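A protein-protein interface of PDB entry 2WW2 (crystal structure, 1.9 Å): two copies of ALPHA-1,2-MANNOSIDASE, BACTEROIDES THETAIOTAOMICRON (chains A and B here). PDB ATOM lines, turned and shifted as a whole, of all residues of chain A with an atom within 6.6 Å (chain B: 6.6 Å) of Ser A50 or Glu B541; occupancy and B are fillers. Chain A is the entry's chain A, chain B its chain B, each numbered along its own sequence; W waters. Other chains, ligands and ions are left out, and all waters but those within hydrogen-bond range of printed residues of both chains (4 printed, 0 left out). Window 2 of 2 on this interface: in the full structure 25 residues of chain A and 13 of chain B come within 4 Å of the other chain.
N of Trp A52 sits close to OG of Ser A50 (3.0 Å).
OG of Ser A50 sits at hydrogen-bond distance from OE1 of Glu B541 (2.6 Å).
Of the 19 printed residues of chain A, 3 touch a printed residue of chain B. Of the 12 printed residues of chain B, 4 touch a printed residue of chain A. Printed residues of chain B that touch a printed residue of chain A: Glu B541, Pro B542, Ala B545 and Arg B546. Hydrophobic or aromatic side chains of chain B that line the printed part of chain A: Ala B545. Among the printed residues, no Asp or Glu carboxylate lies within 4 Å of a Lys or Arg side-chain nitrogen of the other chain.
Ser A50 touches just one residue of chain B: Glu B541. Glu B541 touches just these residues of chain A: Ser A50 and Trp A52. Of the printed residues of chain A, Pro B542 touches Phe A23 (3.8 Å) and Trp A52 (3.9 Å). Printed residues of chain B within 4 Å of Phe A23: Pro B542 (3.8 Å), Ala B545 (3.8 Å) and Arg B546 (3.6 Å). Printed residues of chain B within 4 Å of Trp A52: Glu B541 and Pro B542. Ile B597 touches none of the printed residues of chain A. The nearest printed residue of chain A that does not touch Arg B546 is Trp A52 (6.9 Å).
Water W2 lies within hydrogen-bond range of O of Trp A52 (2.5 Å), OE2 of Glu B541 (2.8 Å) and OG1 of Thr A55 (3.0 Å). Water W4 bridges the side-chain carboxylate of Asp A58 (2.7 Å) and the side-chain amide nitrogen of Gln B599 (3.0 Å). Water W1 bridges N of Glu A47 (2.8 Å) and OE2 of Glu B541 (3.3 Å). Water W3 lies within hydrogen-bond range of the side-chain carboxylate (OD1) of Asp A58 (3.0 Å) and the side-chain amide nitrogen (NE2) of Gln B599 (3.4 Å).
Among the printed residues, merely in contact across the chains: Trp A52 with Glu B541 (3.6 Å), Phe A23 with Arg B546 (3.6 Å), Phe A23 with Ala B545 (3.8 Å), Phe A23 with Pro B542 (3.8 Å) and Trp A52 with Pro B542 (3.9 Å).
No position is printed for both chains. Of the 6 pairs that touch across the chains among the printed residues, none has its exchanged pair printed and touching as well.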
ATOM      1  N   PHE A  23     -10.905  -1.459 -10.933  1.00  0.00           N
ATOM      2  CA  PHE A  23     -12.131  -1.974 -11.535  1.00  0.00           C
ATOM      3  C   PHE A  23     -12.047  -3.473 -11.751  1.00  0.00           C
ATOM      4  O   PHE A  23     -12.398  -3.992 -12.822  1.00  0.00           O
ATOM      5  CB  PHE A  23     -12.457  -1.200 -12.822  1.00  0.00           C
ATOM      6  CG  PHE A  23     -12.701   0.264 -12.572  1.00  0.00           C
ATOM      7  CD1 PHE A  23     -11.656   1.176 -12.636  1.00  0.00           C
ATOM      8  CD2 PHE A  23     -13.959   0.717 -12.209  1.00  0.00           C
ATOM      9  CE1 PHE A  23     -11.876   2.517 -12.380  1.00  0.00           C
ATOM     10  CE2 PHE A  23     -14.178   2.067 -11.949  1.00  0.00           C
ATOM     11  CZ  PHE A  23     -13.141   2.959 -12.038  1.00  0.00           C
ATOM     12  N   GLN A  44     -10.697   0.123   8.451  1.00  0.00           N
ATOM     13  CA  GLN A  44     -11.436   0.804   7.383  1.00  0.00           C
ATOM     14  C   GLN A  44     -10.891   2.231   7.192  1.00  0.00           C
ATOM     15  O   GLN A  44     -10.879   3.032   8.139  1.00  0.00           O
ATOM     16  CB  GLN A  44     -12.930   0.860   7.722  1.00  0.00           C
ATOM     17  CG  GLN A  44     -13.749   1.733   6.748  1.00  0.00           C
ATOM     18  CD  GLN A  44     -15.157   1.983   7.266  1.00  0.00           C
ATOM     19  OE1 GLN A  44     -15.554   1.424   8.291  1.00  0.00           O
ATOM     20  NE2 GLN A  44     -15.918   2.821   6.560  1.00  0.00           N
ATOM     21  N   GLY A  46     -11.780   3.776   3.944  1.00  0.00           N
ATOM     22  CA  GLY A  46     -12.754   4.309   2.980  1.00  0.00           C
ATOM     23  C   GLY A  46     -14.064   4.696   3.672  1.00  0.00           C
ATOM     24  O   GLY A  46     -14.323   4.278   4.800  1.00  0.00           O
ATOM     25  N   GLU A  47     -14.881   5.510   3.006  1.00  0.00           N
ATOM     26  CA  GLU A  47     -16.189   5.874   3.554  1.00  0.00           C
ATOM     27  C   GLU A  47     -17.065   4.640   3.716  1.00  0.00           C
ATOM     28  O   GLU A  47     -16.899   3.680   2.975  1.00  0.00           O
ATOM     29  CB  GLU A  47     -16.910   6.830   2.596  1.00  0.00           C
ATOM     30  CG  GLU A  47     -16.448   8.250   2.680  1.00  0.00           C
ATOM     31  CD  GLU A  47     -17.361   9.194   1.894  1.00  0.00           C
ATOM     32  OE1 GLU A  47     -18.420   8.752   1.380  1.00  0.00           O
ATOM     33  OE2 GLU A  47     -17.007  10.375   1.792  1.00  0.00           O
ATOM     34  N   ASN A  48     -18.033   4.688   4.630  1.00  0.00           N
ATOM     35  CA  ASN A  48     -19.078   3.681   4.648  1.00  0.00           C
ATOM     36  C   ASN A  48     -19.673   3.604   3.247  1.00  0.00           C
ATOM     37  O   ASN A  48     -19.935   4.645   2.632  1.00  0.00           O
ATOM     38  CB  ASN A  48     -20.217   4.051   5.623  1.00  0.00           C
ATOM     39  CG  ASN A  48     -19.839   3.858   7.100  1.00  0.00           C
ATOM     40  OD1 ASN A  48     -18.683   3.584   7.435  1.00  0.00           O
ATOM     41  ND2 ASN A  48     -20.832   3.985   7.983  1.00  0.00           N
ATOM     42  N   GLY A  49     -19.913   2.392   2.762  1.00  0.00           N
ATOM     43  CA  GLY A  49     -20.517   2.206   1.447  1.00  0.00           C
ATOM     44  C   GLY A  49     -19.525   1.956   0.324  1.00  0.00           C
ATOM     45  O   GLY A  49     -19.879   1.415  -0.722  1.00  0.00           O
ATOM     46  N   SER A  50     -18.272   2.341   0.521  1.00  0.00           N
ATOM     47  CA  SER A  50     -17.293   2.128  -0.529  1.00  0.00           C
ATOM     48  C   SER A  50     -16.717   0.710  -0.476  1.00  0.00           C
ATOM     49  O   SER A  50     -16.260   0.267   0.577  1.00  0.00           O
ATOM     50  CB  SER A  50     -16.145   3.134  -0.404  1.00  0.00           C
ATOM     51  OG  SER A  50     -15.115   2.785  -1.320  1.00  0.00           O
ATOM     52  N   GLY A  51     -16.692   0.028  -1.621  1.00  0.00           N
ATOM     53  CA  GLY A  51     -16.060  -1.300  -1.687  1.00  0.00           C
ATOM     54  C   GLY A  51     -14.568  -1.231  -1.429  1.00  0.00           C
ATOM     55  O   GLY A  51     -13.942  -2.236  -1.095  1.00  0.00           O
ATOM     56  N   TRP A  52     -14.000  -0.034  -1.549  1.00  0.00           N
ATOM     57  CA  TRP A  52     -12.576   0.162  -1.292  1.00  0.00           C
ATOM     58  C   TRP A  52     -12.383   0.503   0.194  1.00  0.00           C
ATOM     59  O   TRP A  52     -12.066   1.636   0.593  1.00  0.00           O
ATOM     60  CB  TRP A  52     -12.007   1.228  -2.244  1.00  0.00           C
ATOM     61  CG  TRP A  52     -12.092   0.787  -3.710  1.00  0.00           C
ATOM     62  CD1 TRP A  52     -11.704  -0.423  -4.218  1.00  0.00           C
ATOM     63  CD2 TRP A  52     -12.563   1.558  -4.825  1.00  0.00           C
ATOM     64  NE1 TRP A  52     -11.910  -0.458  -5.583  1.00  0.00           N
ATOM     65  CE2 TRP A  52     -12.434   0.750  -5.978  1.00  0.00           C
ATOM     66  CE3 TRP A  52     -13.074   2.860  -4.966  1.00  0.00           C
ATOM     67  CZ2 TRP A  52     -12.794   1.198  -7.259  1.00  0.00           C
ATOM     68  CZ3 TRP A  52     -13.443   3.308  -6.251  1.00  0.00           C
ATOM     69  CH2 TRP A  52     -13.306   2.467  -7.379  1.00  0.00           C
ATOM     70  N   MET A  53     -12.611  -0.513   1.009  1.00  0.00           N
ATOM     71  CA  MET A  53     -12.715  -0.352   2.448  1.00  0.00           C
ATOM     72  C   MET A  53     -11.394   0.064   3.063  1.00  0.00           C
ATOM     73  O   MET A  53     -11.358   0.880   3.980  1.00  0.00           O
ATOM     74  CB  MET A  53     -13.171  -1.682   3.063  1.00  0.00           C
ATOM     75  CG  MET A  53     -13.197  -1.691   4.579  1.00  0.00           C
ATOM     76  SD  MET A  53     -13.988  -3.204   5.221  1.00  0.00           S
ATOM     77  CE  MET A  53     -13.007  -4.453   4.500  1.00  0.00           C
ATOM     78  N   TYR A  54     -10.315  -0.552   2.601  1.00  0.00           N
ATOM     79  CA  TYR A  54      -8.988  -0.251   3.116  1.00  0.00           C
ATOM     80  C   TYR A  54      -8.118   0.038   1.904  1.00  0.00           C
ATOM     81  O   TYR A  54      -7.950  -0.823   1.043  1.00  0.00           O
ATOM     82  CB  TYR A  54      -8.421  -1.437   3.930  1.00  0.00           C
ATOM     83  CG  TYR A  54      -6.981  -1.254   4.419  1.00  0.00           C
ATOM     84  CD1 TYR A  54      -6.713  -0.764   5.697  1.00  0.00           C
ATOM     85  CD2 TYR A  54      -5.895  -1.589   3.600  1.00  0.00           C
ATOM     86  CE1 TYR A  54      -5.389  -0.600   6.153  1.00  0.00           C
ATOM     87  CE2 TYR A  54      -4.569  -1.428   4.046  1.00  0.00           C
ATOM     88  CZ  TYR A  54      -4.328  -0.939   5.310  1.00  0.00           C
ATOM     89  OH  TYR A  54      -3.028  -0.790   5.741  1.00  0.00           O
ATOM     90  N   THR A  55      -7.572   1.254   1.852  1.00  0.00           N
ATOM     91  CA  THR A  55      -6.690   1.678   0.779  1.00  0.00           C
ATOM     92  C   THR A  55      -5.327   1.973   1.398  1.00  0.00           C
ATOM     93  O   THR A  55      -5.198   2.852   2.256  1.00  0.00           O
ATOM     94  CB  THR A  55      -7.303   2.913   0.072  1.00  0.00           C
ATOM     95  OG1 THR A  55      -8.489   2.495  -0.616  1.00  0.00           O
ATOM     96  CG2 THR A  55      -6.330   3.561  -0.915  1.00  0.00           C
ATOM     97  N   ASP A  58      -4.023   5.463   1.807  1.00  0.00           N
ATOM     98  CA  ASP A  58      -4.775   6.417   2.619  1.00  0.00           C
ATOM     99  C   ASP A  58      -4.283   6.336   4.061  1.00  0.00           C
ATOM    100  O   ASP A  58      -3.945   5.253   4.543  1.00  0.00           O
ATOM    101  CB  ASP A  58      -6.294   6.214   2.472  1.00  0.00           C
ATOM    102  CG  ASP A  58      -6.811   6.729   1.115  1.00  0.00           C
ATOM    103  OD1 ASP A  58      -6.171   7.621   0.515  1.00  0.00           O
ATOM    104  OD2 ASP A  58      -7.839   6.259   0.619  1.00  0.00           O
ATOM    105  N   ARG A  65     -14.118  -2.709  10.998  1.00  0.00           N
ATOM    106  CA  ARG A  65     -15.367  -3.262  10.494  1.00  0.00           C
ATOM    107  C   ARG A  65     -15.456  -4.749  10.727  1.00  0.00           C
ATOM    108  O   ARG A  65     -14.476  -5.480  10.501  1.00  0.00           O
ATOM    109  CB  ARG A  65     -15.433  -3.046   8.976  1.00  0.00           C
ATOM    110  CG  ARG A  65     -15.702  -1.607   8.535  1.00  0.00           C
ATOM    111  CD  ARG A  65     -17.185  -1.399   8.203  1.00  0.00           C
ATOM    112  NE  ARG A  65     -17.560  -2.074   6.963  1.00  0.00           N
ATOM    113  CZ  ARG A  65     -17.210  -1.677   5.741  1.00  0.00           C
ATOM    114  NH1 ARG A  65     -16.450  -0.595   5.563  1.00  0.00           N
ATOM    115  NH2 ARG A  65     -17.624  -2.377   4.689  1.00  0.00           N
ATOM    116  N   GLN A  69     -17.163  -8.833   3.038  1.00  0.00           N
ATOM    117  CA  GLN A  69     -16.987  -8.485   1.610  1.00  0.00           C
ATOM    118  C   GLN A  69     -16.018  -9.401   0.843  1.00  0.00           C
ATOM    119  O   GLN A  69     -14.862  -9.551   1.225  1.00  0.00           O
ATOM    120  CB  GLN A  69     -16.508  -7.042   1.475  1.00  0.00           C
ATOM    121  CG  GLN A  69     -16.166  -6.609   0.051  1.00  0.00           C
ATOM    122  CD  GLN A  69     -15.820  -5.147   0.021  1.00  0.00           C
ATOM    123  OE1 GLN A  69     -16.667  -4.312   0.322  1.00  0.00           O
ATOM    124  NE2 GLN A  69     -14.564  -4.819  -0.293  1.00  0.00           N
ATOM    125  N   PRO A  72     -14.667  -5.735  -3.954  1.00  0.00           N
ATOM    126  CA  PRO A  72     -15.141  -4.353  -3.756  1.00  0.00           C
ATOM    127  C   PRO A  72     -16.367  -4.059  -4.585  1.00  0.00           C
ATOM    128  O   PRO A  72     -17.170  -3.224  -4.195  1.00  0.00           O
ATOM    129  CB  PRO A  72     -13.979  -3.477  -4.235  1.00  0.00           C
ATOM    130  CG  PRO A  72     -12.980  -4.404  -4.878  1.00  0.00           C
ATOM    131  CD  PRO A  72     -13.273  -5.812  -4.424  1.00  0.00           C
ATOM    132  N   ASN A  75     -19.205  -5.833  -2.965  1.00  0.00           N
ATOM    133  CA  ASN A  75     -19.374  -4.968  -1.798  1.00  0.00           C
ATOM    134  C   ASN A  75     -19.860  -5.799  -0.593  1.00  0.00           C
ATOM    135  O   ASN A  75     -19.765  -7.040  -0.612  1.00  0.00           O
ATOM    136  CB  ASN A  75     -20.268  -3.738  -2.158  1.00  0.00           C
ATOM    137  CG  ASN A  75     -19.969  -2.488  -1.288  1.00  0.00           C
ATOM    138  OD1 ASN A  75     -19.900  -2.571  -0.060  1.00  0.00           O
ATOM    139  ND2 ASN A  75     -19.862  -1.328  -1.930  1.00  0.00           N
ATOM    140  N   TYR A 150     -23.997   1.404  10.485  1.00  0.00           N
ATOM    141  CA  TYR A 150     -24.094   1.596   9.029  1.00  0.00           C
ATOM    142  C   TYR A 150     -25.461   2.157   8.635  1.00  0.00           C
ATOM    143  O   TYR A 150     -26.313   2.397   9.497  1.00  0.00           O
ATOM    144  CB  TYR A 150     -23.841   0.278   8.297  1.00  0.00           C
ATOM    145  CG  TYR A 150     -22.689   0.310   7.317  1.00  0.00           C
ATOM    146  CD1 TYR A 150     -22.914   0.269   5.943  1.00  0.00           C
ATOM    147  CD2 TYR A 150     -21.375   0.369   7.760  1.00  0.00           C
ATOM    148  CE1 TYR A 150     -21.855   0.268   5.034  1.00  0.00           C
ATOM    149  CE2 TYR A 150     -20.298   0.385   6.856  1.00  0.00           C
ATOM    150  CZ  TYR A 150     -20.563   0.319   5.495  1.00  0.00           C
ATOM    151  OH  TYR A 150     -19.539   0.290   4.575  1.00  0.00           O
ATOM    152  N   TYR A 171     -27.575  -3.162   6.298  1.00  0.00           N
ATOM    153  CA  TYR A 171     -26.931  -2.750   5.063  1.00  0.00           C
ATOM    154  C   TYR A 171     -26.592  -3.966   4.209  1.00  0.00           C
ATOM    155  O   TYR A 171     -26.134  -4.998   4.723  1.00  0.00           O
ATOM    156  CB  TYR A 171     -25.651  -1.965   5.353  1.00  0.00           C
ATOM    157  CG  TYR A 171     -24.842  -1.639   4.106  1.00  0.00           C
ATOM    158  CD1 TYR A 171     -25.133  -0.520   3.333  1.00  0.00           C
ATOM    159  CD2 TYR A 171     -23.778  -2.453   3.711  1.00  0.00           C
ATOM    160  CE1 TYR A 171     -24.381  -0.223   2.192  1.00  0.00           C
ATOM    161  CE2 TYR A 171     -23.024  -2.172   2.570  1.00  0.00           C
ATOM    162  CZ  TYR A 171     -23.331  -1.043   1.828  1.00  0.00           C
ATOM    163  OH  TYR A 171     -22.596  -0.763   0.722  1.00  0.00           O
ATOM    164  N   SER B 534     -18.262  13.193 -12.837  1.00  0.00           N
ATOM    165  CA  SER B 534     -18.018  12.153 -11.836  1.00  0.00           C
ATOM    166  C   SER B 534     -19.304  11.364 -11.611  1.00  0.00           C
ATOM    167  O   SER B 534     -19.266  10.154 -11.398  1.00  0.00           O
ATOM    168  CB  SER B 534     -17.449  12.716 -10.519  1.00  0.00           C
ATOM    169  OG  SER B 534     -18.438  13.310  -9.696  1.00  0.00           O
ATOM    170  N   GLY B 538     -19.764   7.282 -11.805  1.00  0.00           N
ATOM    171  CA  GLY B 538     -20.174   6.518 -10.633  1.00  0.00           C
ATOM    172  C   GLY B 538     -19.809   7.153  -9.307  1.00  0.00           C
ATOM    173  O   GLY B 538     -20.043   6.556  -8.262  1.00  0.00           O
ATOM    174  N   GLY B 539     -19.228   8.354  -9.350  1.00  0.00           N
ATOM    175  CA  GLY B 539     -18.930   9.109  -8.145  1.00  0.00           C
ATOM    176  C   GLY B 539     -17.501   9.613  -8.095  1.00  0.00           C
ATOM    177  O   GLY B 539     -16.708   9.362  -9.008  1.00  0.00           O
ATOM    178  N   HIS B 540     -17.174  10.323  -7.021  1.00  0.00           N
ATOM    179  CA  HIS B 540     -15.835  10.845  -6.829  1.00  0.00           C
ATOM    180  C   HIS B 540     -14.789   9.735  -6.833  1.00  0.00           C
ATOM    181  O   HIS B 540     -13.761   9.843  -7.495  1.00  0.00           O
ATOM    182  CB  HIS B 540     -15.775  11.616  -5.517  1.00  0.00           C
ATOM    183  CG  HIS B 540     -16.492  12.927  -5.567  1.00  0.00           C
ATOM    184  ND1 HIS B 540     -16.518  13.800  -4.502  1.00  0.00           N
ATOM    185  CD2 HIS B 540     -17.180  13.526  -6.566  1.00  0.00           C
ATOM    186  CE1 HIS B 540     -17.215  14.875  -4.836  1.00  0.00           C
ATOM    187  NE2 HIS B 540     -17.629  14.731  -6.081  1.00  0.00           N
ATOM    188  N   GLU B 541     -15.057   8.658  -6.096  1.00  0.00           N
ATOM    189  CA  GLU B 541     -14.062   7.589  -5.973  1.00  0.00           C
ATOM    190  C   GLU B 541     -13.710   6.906  -7.290  1.00  0.00           C
ATOM    191  O   GLU B 541     -12.546   6.742  -7.601  1.00  0.00           O
ATOM    192  CB  GLU B 541     -14.431   6.571  -4.884  1.00  0.00           C
ATOM    193  CG  GLU B 541     -13.612   6.823  -3.630  1.00  0.00           C
ATOM    194  CD  GLU B 541     -13.582   5.643  -2.672  1.00  0.00           C
ATOM    195  OE1 GLU B 541     -14.648   5.041  -2.447  1.00  0.00           O
ATOM    196  OE2 GLU B 541     -12.489   5.327  -2.145  1.00  0.00           O
ATOM    197  N   PRO B 542     -14.715   6.525  -8.081  1.00  0.00           N
ATOM    198  CA  PRO B 542     -14.400   5.967  -9.384  1.00  0.00           C
ATOM    199  C   PRO B 542     -13.635   6.960 -10.278  1.00  0.00           C
ATOM    200  O   PRO B 542     -12.712   6.564 -10.991  1.00  0.00           O
ATOM    201  CB  PRO B 542     -15.780   5.648  -9.973  1.00  0.00           C
ATOM    202  CG  PRO B 542     -16.646   5.447  -8.771  1.00  0.00           C
ATOM    203  CD  PRO B 542     -16.157   6.472  -7.791  1.00  0.00           C
ATOM    204  N   MET B 543     -14.006   8.238 -10.261  1.00  0.00           N
ATOM    205  CA  MET B 543     -13.258   9.206 -11.069  1.00  0.00           C
ATOM    206  C   MET B 543     -11.805   9.305 -10.605  1.00  0.00           C
ATOM    207  O   MET B 543     -10.879   9.361 -11.423  1.00  0.00           O
ATOM    208  CB  MET B 543     -13.924  10.588 -11.063  1.00  0.00           C
ATOM    209  CG  MET B 543     -13.116  11.622 -11.861  1.00  0.00           C
ATOM    210  SD  MET B 543     -13.780  13.302 -11.821  1.00  0.00           S
ATOM    211  CE  MET B 543     -14.971  13.231 -13.160  1.00  0.00           C
ATOM    212  N   ILE B 544     -11.594   9.322  -9.296  1.00  0.00           N
ATOM    213  CA  ILE B 544     -10.238   9.267  -8.757  1.00  0.00           C
ATOM    214  C   ILE B 544      -9.484   8.042  -9.285  1.00  0.00           C
ATOM    215  O   ILE B 544      -8.358   8.149  -9.755  1.00  0.00           O
ATOM    216  CB  ILE B 544     -10.258   9.249  -7.215  1.00  0.00           C
ATOM    217  CG1 ILE B 544     -10.762  10.604  -6.693  1.00  0.00           C
ATOM    218  CG2 ILE B 544      -8.862   8.877  -6.635  1.00  0.00           C
ATOM    219  CD1 ILE B 544     -11.173  10.553  -5.238  1.00  0.00           C
ATOM    220  N   ALA B 545     -10.128   6.876  -9.222  1.00  0.00           N
ATOM    221  CA  ALA B 545      -9.512   5.634  -9.677  1.00  0.00           C
ATOM    222  C   ALA B 545      -9.064   5.723 -11.136  1.00  0.00           C
ATOM    223  O   ALA B 545      -7.962   5.291 -11.485  1.00  0.00           O
ATOM    224  CB  ALA B 545     -10.477   4.452  -9.466  1.00  0.00           C
ATOM    225  N   ARG B 546      -9.902   6.317 -11.982  1.00  0.00           N
ATOM    226  CA  ARG B 546      -9.588   6.470 -13.410  1.00  0.00           C
ATOM    227  C   ARG B 546      -8.476   7.485 -13.693  1.00  0.00           C
ATOM    228  O   ARG B 546      -7.610   7.261 -14.545  1.00  0.00           O
ATOM    229  CB  ARG B 546     -10.849   6.818 -14.196  1.00  0.00           C
ATOM    230  CG  ARG B 546     -11.900   5.713 -14.132  1.00  0.00           C
ATOM    231  CD  ARG B 546     -13.189   6.110 -14.832  1.00  0.00           C
ATOM    232  NE  ARG B 546     -12.994   6.245 -16.271  1.00  0.00           N
ATOM    233  CZ  ARG B 546     -13.987   6.212 -17.155  1.00  0.00           C
ATOM    234  NH1 ARG B 546     -15.234   6.042 -16.739  1.00  0.00           N
ATOM    235  NH2 ARG B 546     -13.728   6.345 -18.450  1.00  0.00           N
ATOM    236  N   ILE B 597     -12.759  16.634  -6.396  1.00  0.00           N
ATOM    237  CA  ILE B 597     -13.313  15.358  -5.937  1.00  0.00           C
ATOM    238  C   ILE B 597     -12.658  14.856  -4.655  1.00  0.00           C
ATOM    239  O   ILE B 597     -12.770  13.683  -4.327  1.00  0.00           O
ATOM    240  CB  ILE B 597     -13.253  14.265  -7.055  1.00  0.00           C
ATOM    241  CG1 ILE B 597     -11.808  14.045  -7.544  1.00  0.00           C
ATOM    242  CG2 ILE B 597     -14.129  14.675  -8.235  1.00  0.00           C
ATOM    243  CD1 ILE B 597     -11.693  13.240  -8.859  1.00  0.00           C
ATOM    244  N   GLN B 599      -9.236  15.060  -3.362  1.00  0.00           N
ATOM    245  CA  GLN B 599      -7.843  14.639  -3.155  1.00  0.00           C
ATOM    246  C   GLN B 599      -6.804  15.541  -3.820  1.00  0.00           C
ATOM    247  O   GLN B 599      -6.038  15.095  -4.670  1.00  0.00           O
ATOM    248  CB  GLN B 599      -7.650  13.177  -3.576  1.00  0.00           C
ATOM    249  CG  GLN B 599      -8.544  12.193  -2.810  1.00  0.00           C
ATOM    250  CD  GLN B 599      -8.149  10.758  -3.059  1.00  0.00           C
ATOM    251  OE1 GLN B 599      -7.464  10.458  -4.035  1.00  0.00           O
ATOM    252  NE2 GLN B 599      -8.576   9.863  -2.180  1.00  0.00           N
HETATM  253  O   HOH W   1     -14.110   6.454   0.509  1.00  0.00           O
HETATM  254  O   HOH W   2     -11.169   3.814  -0.236  1.00  0.00           O
HETATM  255  O   HOH W   3      -8.625   9.293   1.185  1.00  0.00           O
HETATM  256  O   HOH W   4      -8.647   6.855  -1.920  1.00  0.00           O
